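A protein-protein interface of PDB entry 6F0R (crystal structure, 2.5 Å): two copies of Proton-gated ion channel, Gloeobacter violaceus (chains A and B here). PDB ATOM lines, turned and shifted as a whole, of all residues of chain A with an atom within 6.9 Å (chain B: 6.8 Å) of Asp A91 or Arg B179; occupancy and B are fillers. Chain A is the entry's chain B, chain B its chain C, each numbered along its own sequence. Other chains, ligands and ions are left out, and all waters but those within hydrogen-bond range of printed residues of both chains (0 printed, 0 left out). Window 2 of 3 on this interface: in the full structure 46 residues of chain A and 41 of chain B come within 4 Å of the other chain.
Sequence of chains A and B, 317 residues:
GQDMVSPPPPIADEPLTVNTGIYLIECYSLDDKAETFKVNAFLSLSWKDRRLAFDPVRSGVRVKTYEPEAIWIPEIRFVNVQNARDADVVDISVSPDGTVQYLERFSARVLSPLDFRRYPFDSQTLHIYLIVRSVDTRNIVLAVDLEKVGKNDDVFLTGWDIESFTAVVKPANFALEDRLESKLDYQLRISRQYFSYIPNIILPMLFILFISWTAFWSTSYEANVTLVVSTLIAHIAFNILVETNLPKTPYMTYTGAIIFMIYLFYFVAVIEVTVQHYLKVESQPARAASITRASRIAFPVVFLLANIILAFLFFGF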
ATOM      1  N   VAL A  63     -10.944  12.425   1.911  1.00  0.00           N
ATOM      2  CA  VAL A  63     -12.312  12.961   1.938  1.00  0.00           C
ATOM      3  C   VAL A  63     -12.243  14.467   2.207  1.00  0.00           C
ATOM      4  O   VAL A  63     -11.425  14.900   3.024  1.00  0.00           O
ATOM      5  CB  VAL A  63     -13.206  12.259   2.985  1.00  0.00           C
ATOM      6  CG1 VAL A  63     -13.954  11.096   2.370  1.00  0.00           C
ATOM      7  CG2 VAL A  63     -12.407  11.807   4.201  1.00  0.00           C
ATOM      8  N   LYS A  64     -13.091  15.259   1.524  1.00  0.00           N
ATOM      9  CA  LYS A  64     -13.116  16.716   1.671  1.00  0.00           C
ATOM     10  C   LYS A  64     -14.390  17.203   2.300  1.00  0.00           C
ATOM     11  O   LYS A  64     -15.477  16.872   1.820  1.00  0.00           O
ATOM     12  CB  LYS A  64     -12.909  17.418   0.320  1.00  0.00           C
ATOM     13  CG  LYS A  64     -11.493  17.347  -0.215  1.00  0.00           C
ATOM     14  CD  LYS A  64     -11.453  17.917  -1.626  1.00  0.00           C
ATOM     15  CE  LYS A  64     -10.081  17.934  -2.194  1.00  0.00           C
ATOM     16  NZ  LYS A  64     -10.095  18.398  -3.602  1.00  0.00           N
ATOM     17  N   THR A  65     -14.261  18.001   3.373  1.00  0.00           N
ATOM     18  CA  THR A  65     -15.400  18.591   4.082  1.00  0.00           C
ATOM     19  C   THR A  65     -15.728  19.942   3.447  1.00  0.00           C
ATOM     20  O   THR A  65     -14.821  20.722   3.187  1.00  0.00           O
ATOM     21  CB  THR A  65     -15.140  18.680   5.596  1.00  0.00           C
ATOM     22  OG1 THR A  65     -14.401  17.543   6.042  1.00  0.00           O
ATOM     23  CG2 THR A  65     -16.411  18.771   6.386  1.00  0.00           C
ATOM     24  N   TYR A  66     -17.007  20.207   3.173  1.00  0.00           N
ATOM     25  CA  TYR A  66     -17.425  21.462   2.549  1.00  0.00           C
ATOM     26  C   TYR A  66     -18.513  22.169   3.351  1.00  0.00           C
ATOM     27  O   TYR A  66     -19.298  21.522   4.056  1.00  0.00           O
ATOM     28  CB  TYR A  66     -17.975  21.217   1.134  1.00  0.00           C
ATOM     29  CG  TYR A  66     -16.945  21.037   0.048  1.00  0.00           C
ATOM     30  CD1 TYR A  66     -16.555  19.770  -0.361  1.00  0.00           C
ATOM     31  CD2 TYR A  66     -16.436  22.131  -0.643  1.00  0.00           C
ATOM     32  CE1 TYR A  66     -15.656  19.592  -1.408  1.00  0.00           C
ATOM     33  CE2 TYR A  66     -15.520  21.968  -1.680  1.00  0.00           C
ATOM     34  CZ  TYR A  66     -15.140  20.694  -2.065  1.00  0.00           C
ATOM     35  OH  TYR A  66     -14.262  20.517  -3.101  1.00  0.00           O
ATOM     36  N   ASP A  88     -29.870  22.240  10.741  1.00  0.00           N
ATOM     37  CA  ASP A  88     -28.501  22.585  11.100  1.00  0.00           C
ATOM     38  C   ASP A  88     -27.631  21.523  10.434  1.00  0.00           C
ATOM     39  O   ASP A  88     -27.767  20.343  10.760  1.00  0.00           O
ATOM     40  CB  ASP A  88     -28.298  22.631  12.642  1.00  0.00           C
ATOM     41  CG  ASP A  88     -26.857  22.397  13.128  1.00  0.00           C
ATOM     42  OD1 ASP A  88     -25.904  23.040  12.564  1.00  0.00           O
ATOM     43  OD2 ASP A  88     -26.675  21.598  14.077  1.00  0.00           O
ATOM     44  N   VAL A  89     -26.772  21.917   9.469  1.00  0.00           N
ATOM     45  CA  VAL A  89     -25.926  20.933   8.794  1.00  0.00           C
ATOM     46  C   VAL A  89     -24.860  20.444   9.791  1.00  0.00           C
ATOM     47  O   VAL A  89     -24.351  21.235  10.594  1.00  0.00           O
ATOM     48  CB  VAL A  89     -25.380  21.340   7.397  1.00  0.00           C
ATOM     49  CG1 VAL A  89     -26.496  21.824   6.480  1.00  0.00           C
ATOM     50  CG2 VAL A  89     -24.287  22.376   7.489  1.00  0.00           C
ATOM     51  N   VAL A  90     -24.664  19.121   9.837  1.00  0.00           N
ATOM     52  CA  VAL A  90     -23.733  18.420  10.727  1.00  0.00           C
ATOM     53  C   VAL A  90     -22.441  18.144   9.968  1.00  0.00           C
ATOM     54  O   VAL A  90     -21.355  18.423  10.478  1.00  0.00           O
ATOM     55  CB  VAL A  90     -24.369  17.122  11.312  1.00  0.00           C
ATOM     56  CG1 VAL A  90     -23.374  16.329  12.163  1.00  0.00           C
ATOM     57  CG2 VAL A  90     -25.626  17.440  12.117  1.00  0.00           C
ATOM     58  N   ASP A  91     -22.554  17.584   8.751  1.00  0.00           N
ATOM     59  CA  ASP A  91     -21.404  17.263   7.932  1.00  0.00           C
ATOM     60  C   ASP A  91     -21.752  17.147   6.460  1.00  0.00           C
ATOM     61  O   ASP A  91     -22.868  16.755   6.113  1.00  0.00           O
ATOM     62  CB  ASP A  91     -20.724  15.983   8.445  1.00  0.00           C
ATOM     63  CG  ASP A  91     -19.314  15.810   7.940  1.00  0.00           C
ATOM     64  OD1 ASP A  91     -18.466  16.717   8.196  1.00  0.00           O
ATOM     65  OD2 ASP A  91     -19.045  14.777   7.294  1.00  0.00           O
ATOM     66  N   ILE A  92     -20.808  17.551   5.611  1.00  0.00           N
ATOM     67  CA  ILE A  92     -20.825  17.422   4.157  1.00  0.00           C
ATOM     68  C   ILE A  92     -19.451  16.853   3.814  1.00  0.00           C
ATOM     69  O   ILE A  92     -18.444  17.512   4.042  1.00  0.00           O
ATOM     70  CB  ILE A  92     -21.108  18.732   3.381  1.00  0.00           C
ATOM     71  CG1 ILE A  92     -22.454  19.320   3.754  1.00  0.00           C
ATOM     72  CG2 ILE A  92     -21.024  18.488   1.865  1.00  0.00           C
ATOM     73  CD1 ILE A  92     -22.630  20.744   3.397  1.00  0.00           C
ATOM     74  N   SER A  93     -19.421  15.594   3.358  1.00  0.00           N
ATOM     75  CA  SER A  93     -18.183  14.910   3.038  1.00  0.00           C
ATOM     76  C   SER A  93     -18.184  14.405   1.607  1.00  0.00           C
ATOM     77  O   SER A  93     -19.061  13.623   1.213  1.00  0.00           O
ATOM     78  CB  SER A  93     -17.881  13.804   4.046  1.00  0.00           C
ATOM     79  OG  SER A  93     -17.200  14.345   5.171  1.00  0.00           O
ATOM     80  N   VAL A  94     -17.201  14.900   0.830  1.00  0.00           N
ATOM     81  CA  VAL A  94     -17.020  14.566  -0.574  1.00  0.00           C
ATOM     82  C   VAL A  94     -15.913  13.519  -0.723  1.00  0.00           C
ATOM     83  O   VAL A  94     -14.789  13.692  -0.234  1.00  0.00           O
ATOM     84  CB  VAL A  94     -16.804  15.822  -1.456  1.00  0.00           C
ATOM     85  CG1 VAL A  94     -16.413  15.456  -2.884  1.00  0.00           C
ATOM     86  CG2 VAL A  94     -18.047  16.691  -1.461  1.00  0.00           C
ATOM     87  N   GLN A 101     -21.784  13.217   0.736  1.00  0.00           N
ATOM     88  CA  GLN A 101     -22.520  12.617   1.851  1.00  0.00           C
ATOM     89  C   GLN A 101     -22.865  13.725   2.836  1.00  0.00           C
ATOM     90  O   GLN A 101     -22.005  14.226   3.565  1.00  0.00           O
ATOM     91  CB  GLN A 101     -21.786  11.416   2.477  1.00  0.00           C
ATOM     92  CG  GLN A 101     -21.949  10.149   1.637  1.00  0.00           C
ATOM     93  CD  GLN A 101     -21.890   8.884   2.451  1.00  0.00           C
ATOM     94  OE1 GLN A 101     -20.866   8.567   3.069  1.00  0.00           O
ATOM     95  NE2 GLN A 101     -22.985   8.107   2.431  1.00  0.00           N
ATOM     96  N   TYR A 102     -24.113  14.183   2.731  1.00  0.00           N
ATOM     97  CA  TYR A 102     -24.699  15.273   3.487  1.00  0.00           C
ATOM     98  C   TYR A 102     -25.459  14.721   4.694  1.00  0.00           C
ATOM     99  O   TYR A 102     -26.116  13.675   4.600  1.00  0.00           O
ATOM    100  CB  TYR A 102     -25.637  16.059   2.547  1.00  0.00           C
ATOM    101  CG  TYR A 102     -26.498  17.112   3.197  1.00  0.00           C
ATOM    102  CD1 TYR A 102     -27.709  16.775   3.811  1.00  0.00           C
ATOM    103  CD2 TYR A 102     -26.145  18.458   3.142  1.00  0.00           C
ATOM    104  CE1 TYR A 102     -28.515  17.746   4.402  1.00  0.00           C
ATOM    105  CE2 TYR A 102     -26.945  19.436   3.729  1.00  0.00           C
ATOM    106  CZ  TYR A 102     -28.123  19.075   4.365  1.00  0.00           C
ATOM    107  OH  TYR A 102     -28.904  20.045   4.917  1.00  0.00           O
ATOM    108  N   LEU A 103     -25.380  15.442   5.822  1.00  0.00           N
ATOM    109  CA  LEU A 103     -26.087  15.120   7.049  1.00  0.00           C
ATOM    110  C   LEU A 103     -26.519  16.386   7.776  1.00  0.00           C
ATOM    111  O   LEU A 103     -25.710  17.259   8.056  1.00  0.00           O
ATOM    112  CB  LEU A 103     -25.280  14.187   7.979  1.00  0.00           C
ATOM    113  CG  LEU A 103     -26.009  13.704   9.259  1.00  0.00           C
ATOM    114  CD1 LEU A 103     -27.176  12.761   8.939  1.00  0.00           C
ATOM    115  CD2 LEU A 103     -25.053  13.045  10.223  1.00  0.00           C
ATOM    116  N   GLU A 104     -27.796  16.472   8.098  1.00  0.00           N
ATOM    117  CA  GLU A 104     -28.347  17.592   8.845  1.00  0.00           C
ATOM    118  C   GLU A 104     -29.165  17.052   9.972  1.00  0.00           C
ATOM    119  O   GLU A 104     -29.655  15.928   9.884  1.00  0.00           O
ATOM    120  CB  GLU A 104     -29.223  18.497   7.949  1.00  0.00           C
ATOM    121  CG  GLU A 104     -30.486  17.847   7.409  1.00  0.00           C
ATOM    122  CD  GLU A 104     -31.555  18.813   6.953  1.00  0.00           C
ATOM    123  OE1 GLU A 104     -31.318  19.569   5.981  1.00  0.00           O
ATOM    124  OE2 GLU A 104     -32.634  18.830   7.585  1.00  0.00           O
ATOM    125  N   GLU B  75     -18.495  20.230  16.942  1.00  0.00           N
ATOM    126  CA  GLU B  75     -19.945  20.387  16.904  1.00  0.00           C
ATOM    127  C   GLU B  75     -20.517  19.495  18.002  1.00  0.00           C
ATOM    128  O   GLU B  75     -20.580  18.262  17.844  1.00  0.00           O
ATOM    129  CB  GLU B  75     -20.535  19.971  15.550  1.00  0.00           C
ATOM    130  CG  GLU B  75     -20.129  20.795  14.343  1.00  0.00           C
ATOM    131  CD  GLU B  75     -20.472  20.156  13.005  1.00  0.00           C
ATOM    132  OE1 GLU B  75     -21.252  19.173  12.980  1.00  0.00           O
ATOM    133  OE2 GLU B  75     -19.948  20.636  11.974  1.00  0.00           O
ATOM    134  N   ARG B 133     -20.291  14.033  17.156  1.00  0.00           N
ATOM    135  CA  ARG B 133     -20.199  13.087  16.057  1.00  0.00           C
ATOM    136  C   ARG B 133     -18.776  13.140  15.488  1.00  0.00           C
ATOM    137  O   ARG B 133     -18.264  14.223  15.121  1.00  0.00           O
ATOM    138  CB  ARG B 133     -21.266  13.365  14.990  1.00  0.00           C
ATOM    139  CG  ARG B 133     -21.351  12.256  13.967  1.00  0.00           C
ATOM    140  CD  ARG B 133     -22.479  12.451  12.978  1.00  0.00           C
ATOM    141  NE  ARG B 133     -22.423  11.459  11.900  1.00  0.00           N
ATOM    142  CZ  ARG B 133     -22.993  10.259  11.948  1.00  0.00           C
ATOM    143  NH1 ARG B 133     -23.668   9.882  13.023  1.00  0.00           N
ATOM    144  NH2 ARG B 133     -22.890   9.427  10.919  1.00  0.00           N
ATOM    145  N   SER B 134     -18.124  11.969  15.464  1.00  0.00           N
ATOM    146  CA  SER B 134     -16.765  11.806  14.944  1.00  0.00           C
ATOM    147  C   SER B 134     -16.692  12.136  13.462  1.00  0.00           C
ATOM    148  O   SER B 134     -17.660  11.930  12.729  1.00  0.00           O
ATOM    149  CB  SER B 134     -16.269  10.382  15.174  1.00  0.00           C
ATOM    150  OG  SER B 134     -15.999  10.142  16.546  1.00  0.00           O
ATOM    151  N   VAL B 135     -15.544  12.669  13.035  1.00  0.00           N
ATOM    152  CA  VAL B 135     -15.291  13.041  11.642  1.00  0.00           C
ATOM    153  C   VAL B 135     -14.432  11.961  10.969  1.00  0.00           C
ATOM    154  O   VAL B 135     -13.892  11.087  11.656  1.00  0.00           O
ATOM    155  CB  VAL B 135     -14.702  14.470  11.500  1.00  0.00           C
ATOM    156  CG1 VAL B 135     -15.655  15.529  12.065  1.00  0.00           C
ATOM    157  CG2 VAL B 135     -13.323  14.579  12.148  1.00  0.00           C
ATOM    158  N   ASP B 136     -14.313  12.002   9.643  1.00  0.00           N
ATOM    159  CA  ASP B 136     -13.514  10.986   8.955  1.00  0.00           C
ATOM    160  C   ASP B 136     -12.016  11.052   9.287  1.00  0.00           C
ATOM    161  O   ASP B 136     -11.359  10.006   9.387  1.00  0.00           O
ATOM    162  CB  ASP B 136     -13.753  11.007   7.446  1.00  0.00           C
ATOM    163  CG  ASP B 136     -13.742   9.622   6.866  1.00  0.00           C
ATOM    164  OD1 ASP B 136     -12.643   9.065   6.709  1.00  0.00           O
ATOM    165  OD2 ASP B 136     -14.841   9.081   6.579  1.00  0.00           O
ATOM    166  N   THR B 137     -11.504  12.275   9.509  1.00  0.00           N
ATOM    167  CA  THR B 137     -10.104  12.515   9.855  1.00  0.00           C
ATOM    168  C   THR B 137      -9.781  12.089  11.287  1.00  0.00           C
ATOM    169  O   THR B 137      -8.658  11.658  11.537  1.00  0.00           O
ATOM    170  CB  THR B 137      -9.691  13.965   9.561  1.00  0.00           C
ATOM    171  OG1 THR B 137     -10.812  14.821   9.797  1.00  0.00           O
ATOM    172  CG2 THR B 137      -9.199  14.148   8.135  1.00  0.00           C
ATOM    173  N   ASN B 139     -11.623  10.490  15.279  1.00  0.00           N
ATOM    174  CA  ASN B 139     -12.659  10.048  16.196  1.00  0.00           C
ATOM    175  C   ASN B 139     -12.646  10.972  17.411  1.00  0.00           C
ATOM    176  O   ASN B 139     -11.582  11.256  17.952  1.00  0.00           O
ATOM    177  CB  ASN B 139     -12.440   8.588  16.557  1.00  0.00           C
ATOM    178  CG  ASN B 139     -13.027   7.676  15.518  1.00  0.00           C
ATOM    179  OD1 ASN B 139     -12.705   7.740  14.329  1.00  0.00           O
ATOM    180  ND2 ASN B 139     -13.980   6.870  15.928  1.00  0.00           N
ATOM    181  N   PHE B 174     -20.559   4.795  20.802  1.00  0.00           N
ATOM    182  CA  PHE B 174     -21.309   3.878  19.935  1.00  0.00           C
ATOM    183  C   PHE B 174     -21.324   4.332  18.479  1.00  0.00           C
ATOM    184  O   PHE B 174     -21.099   5.508  18.208  1.00  0.00           O
ATOM    185  CB  PHE B 174     -22.768   3.726  20.455  1.00  0.00           C
ATOM    186  CG  PHE B 174     -23.597   4.994  20.457  1.00  0.00           C
ATOM    187  CD1 PHE B 174     -23.534   5.884  21.524  1.00  0.00           C
ATOM    188  CD2 PHE B 174     -24.439   5.296  19.395  1.00  0.00           C
ATOM    189  CE1 PHE B 174     -24.269   7.077  21.511  1.00  0.00           C
ATOM    190  CE2 PHE B 174     -25.175   6.482  19.381  1.00  0.00           C
ATOM    191  CZ  PHE B 174     -25.087   7.366  20.442  1.00  0.00           C
ATOM    192  N   ALA B 175     -21.643   3.410  17.551  1.00  0.00           N
ATOM    193  CA  ALA B 175     -21.738   3.702  16.121  1.00  0.00           C
ATOM    194  C   ALA B 175     -23.165   4.089  15.733  1.00  0.00           C
ATOM    195  O   ALA B 175     -24.129   3.468  16.185  1.00  0.00           O
ATOM    196  CB  ALA B 175     -21.289   2.500  15.308  1.00  0.00           C
ATOM    197  N   LEU B 176     -23.280   5.120  14.885  1.00  0.00           N
ATOM    198  CA  LEU B 176     -24.539   5.641  14.366  1.00  0.00           C
ATOM    199  C   LEU B 176     -24.266   6.189  12.964  1.00  0.00           C
ATOM    200  O   LEU B 176     -23.490   7.136  12.820  1.00  0.00           O
ATOM    201  CB  LEU B 176     -25.114   6.718  15.308  1.00  0.00           C
ATOM    202  CG  LEU B 176     -26.404   7.413  14.891  1.00  0.00           C
ATOM    203  CD1 LEU B 176     -27.471   6.430  14.565  1.00  0.00           C
ATOM    204  CD2 LEU B 176     -26.865   8.376  15.959  1.00  0.00           C
ATOM    205  N   GLU B 177     -24.871   5.546  11.929  1.00  0.00           N
ATOM    206  CA  GLU B 177     -24.726   5.873  10.498  1.00  0.00           C
ATOM    207  C   GLU B 177     -23.240   5.893  10.094  1.00  0.00           C
ATOM    208  O   GLU B 177     -22.711   6.871   9.542  1.00  0.00           O
ATOM    209  CB  GLU B 177     -25.505   7.148  10.088  1.00  0.00           C
ATOM    210  CG  GLU B 177     -27.024   7.029  10.254  1.00  0.00           C
ATOM    211  CD  GLU B 177     -27.914   8.085   9.613  1.00  0.00           C
ATOM    212  OE1 GLU B 177     -29.155   7.914   9.646  1.00  0.00           O
ATOM    213  OE2 GLU B 177     -27.377   9.073   9.058  1.00  0.00           O
ATOM    214  N   ASP B 178     -22.574   4.765  10.425  1.00  0.00           N
ATOM    215  CA  ASP B 178     -21.173   4.429  10.161  1.00  0.00           C
ATOM    216  C   ASP B 178     -20.177   5.515  10.574  1.00  0.00           C
ATOM    217  O   ASP B 178     -19.256   5.814   9.826  1.00  0.00           O
ATOM    218  CB  ASP B 178     -20.985   4.020   8.687  1.00  0.00           C
ATOM    219  CG  ASP B 178     -19.988   2.892   8.491  1.00  0.00           C
ATOM    220  OD1 ASP B 178     -20.244   1.779   9.008  1.00  0.00           O
ATOM    221  OD2 ASP B 178     -18.973   3.106   7.774  1.00  0.00           O
ATOM    222  N   ARG B 179     -20.364   6.090  11.775  1.00  0.00           N
ATOM    223  CA  ARG B 179     -19.517   7.101  12.440  1.00  0.00           C
ATOM    224  C   ARG B 179     -19.738   6.995  13.952  1.00  0.00           C
ATOM    225  O   ARG B 179     -20.866   6.754  14.394  1.00  0.00           O
ATOM    226  CB  ARG B 179     -19.827   8.546  11.980  1.00  0.00           C
ATOM    227  CG  ARG B 179     -19.369   8.932  10.582  1.00  0.00           C
ATOM    228  CD  ARG B 179     -17.924   9.429  10.537  1.00  0.00           C
ATOM    229  NE  ARG B 179     -17.400   9.551   9.168  1.00  0.00           N
ATOM    230  CZ  ARG B 179     -17.570  10.622   8.394  1.00  0.00           C
ATOM    231  NH1 ARG B 179     -18.248  11.672   8.838  1.00  0.00           N
ATOM    232  NH2 ARG B 179     -17.075  10.645   7.167  1.00  0.00           N
ATOM    233  N   LEU B 180     -18.663   7.162  14.738  1.00  0.00           N
ATOM    234  CA  LEU B 180     -18.712   7.105  16.203  1.00  0.00           C
ATOM    235  C   LEU B 180     -19.403   8.349  16.790  1.00  0.00           C
ATOM    236  O   LEU B 180     -19.209   9.470  16.324  1.00  0.00           O
ATOM    237  CB  LEU B 180     -17.293   6.953  16.783  1.00  0.00           C
ATOM    238  CG  LEU B 180     -17.135   6.680  18.295  1.00  0.00           C
ATOM    239  CD1 LEU B 180     -15.996   5.739  18.557  1.00  0.00           C
ATOM    240  CD2 LEU B 180     -16.853   7.962  19.070  1.00  0.00           C
ATOM    241  N   GLU B 181     -20.185   8.134  17.831  1.00  0.00           N
ATOM    242  CA  GLU B 181     -20.871   9.180  18.563  1.00  0.00           C
ATOM    243  C   GLU B 181     -20.447   9.020  20.022  1.00  0.00           C
ATOM    244  O   GLU B 181     -20.319   7.888  20.492  1.00  0.00           O
ATOM    245  CB  GLU B 181     -22.388   9.043  18.391  1.00  0.00           C
ATOM    246  CG  GLU B 181     -22.888   9.306  16.977  1.00  0.00           C
ATOM    247  CD  GLU B 181     -23.578  10.638  16.722  1.00  0.00           C
ATOM    248  OE1 GLU B 181     -24.000  10.852  15.564  1.00  0.00           O
ATOM    249  OE2 GLU B 181     -23.720  11.455  17.665  1.00  0.00           O
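No position is printed for both chains.
Of the 15 printed residues of chain A, 4 touch a printed residue of chain B. Hydrophobic or aromatic side chains of chain A within 4 Å of the printed part of chain B: Val A63, Val A90 and Leu A103. Printed residues of chain B that touch a printed residue of chain A: Glu B75, Arg B133, Asp B136, Glu B177 and Arg B179. Among the printed residues, Asp or Glu carboxylates within 4 Å of a Lys or Arg side-chain nitrogen of the other chain: Asp A91 with Arg B179 (3.6 Å).
The backbone carbonyl oxygen of Val A90 lies close to the side-chain carboxylate of Glu B75 (2.6 Å). OD2 of Asp A91 lies within salt-bridge range of NH1 of Arg B179, at 3.6 Å.
Among the printed residues, pairs that only touch across the chains: Val A63 with Asp B136 (3.6 Å), Leu A103 with Arg B133 (3.5 Å) and Leu A103 with Glu B177 (3.7 Å).
O of Leu B176 lies within hydrogen-bond range of NH1 of Arg B133 (2.8 Å). O of Asp A91 sits at hydrogen-bond distance from N of Leu A103 (2.8 Å). NH2 of Arg B133 lies within hydrogen-bond range of O of Glu B177 (2.9 Å). The guanidinium group of Arg B133 lies within salt-bridge range of the side-chain carboxylate of Glu B181, 2.7 Å away. The backbone NH (N) of Val A90 lies within hydrogen-bond range of the backbone carbonyl oxygen (O) of Leu A103 (2.8 Å). The side-chain carboxylate (OD2) of Asp A91 is in hydrogen-bond range of the side-chain hydroxyl (OG) of Ser A93 (2.8 Å).
Lys A64 touches none of the printed residues of chain B. Tyr A66 touches none of the printed residues of chain B. Asp A91 touches just one residue of chain B: Arg B179 (3.6 Å). Of the printed residues of chain B, Leu A103 touches Arg B133 (3.5 Å) and Glu B177 (3.7 Å). Of the printed residues of chain A, Glu B75 touches Val A90 (2.6 Å). Printed residues of chain A within 4 Å of Glu B177: Leu A103 (3.7 Å). The nearest residue of chain B that does not touch Asp A91 is Glu B75 (4.7 Å). The nearest printed residue of chain B that does not touch Val A63 is Thr B137 (5.4 Å).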
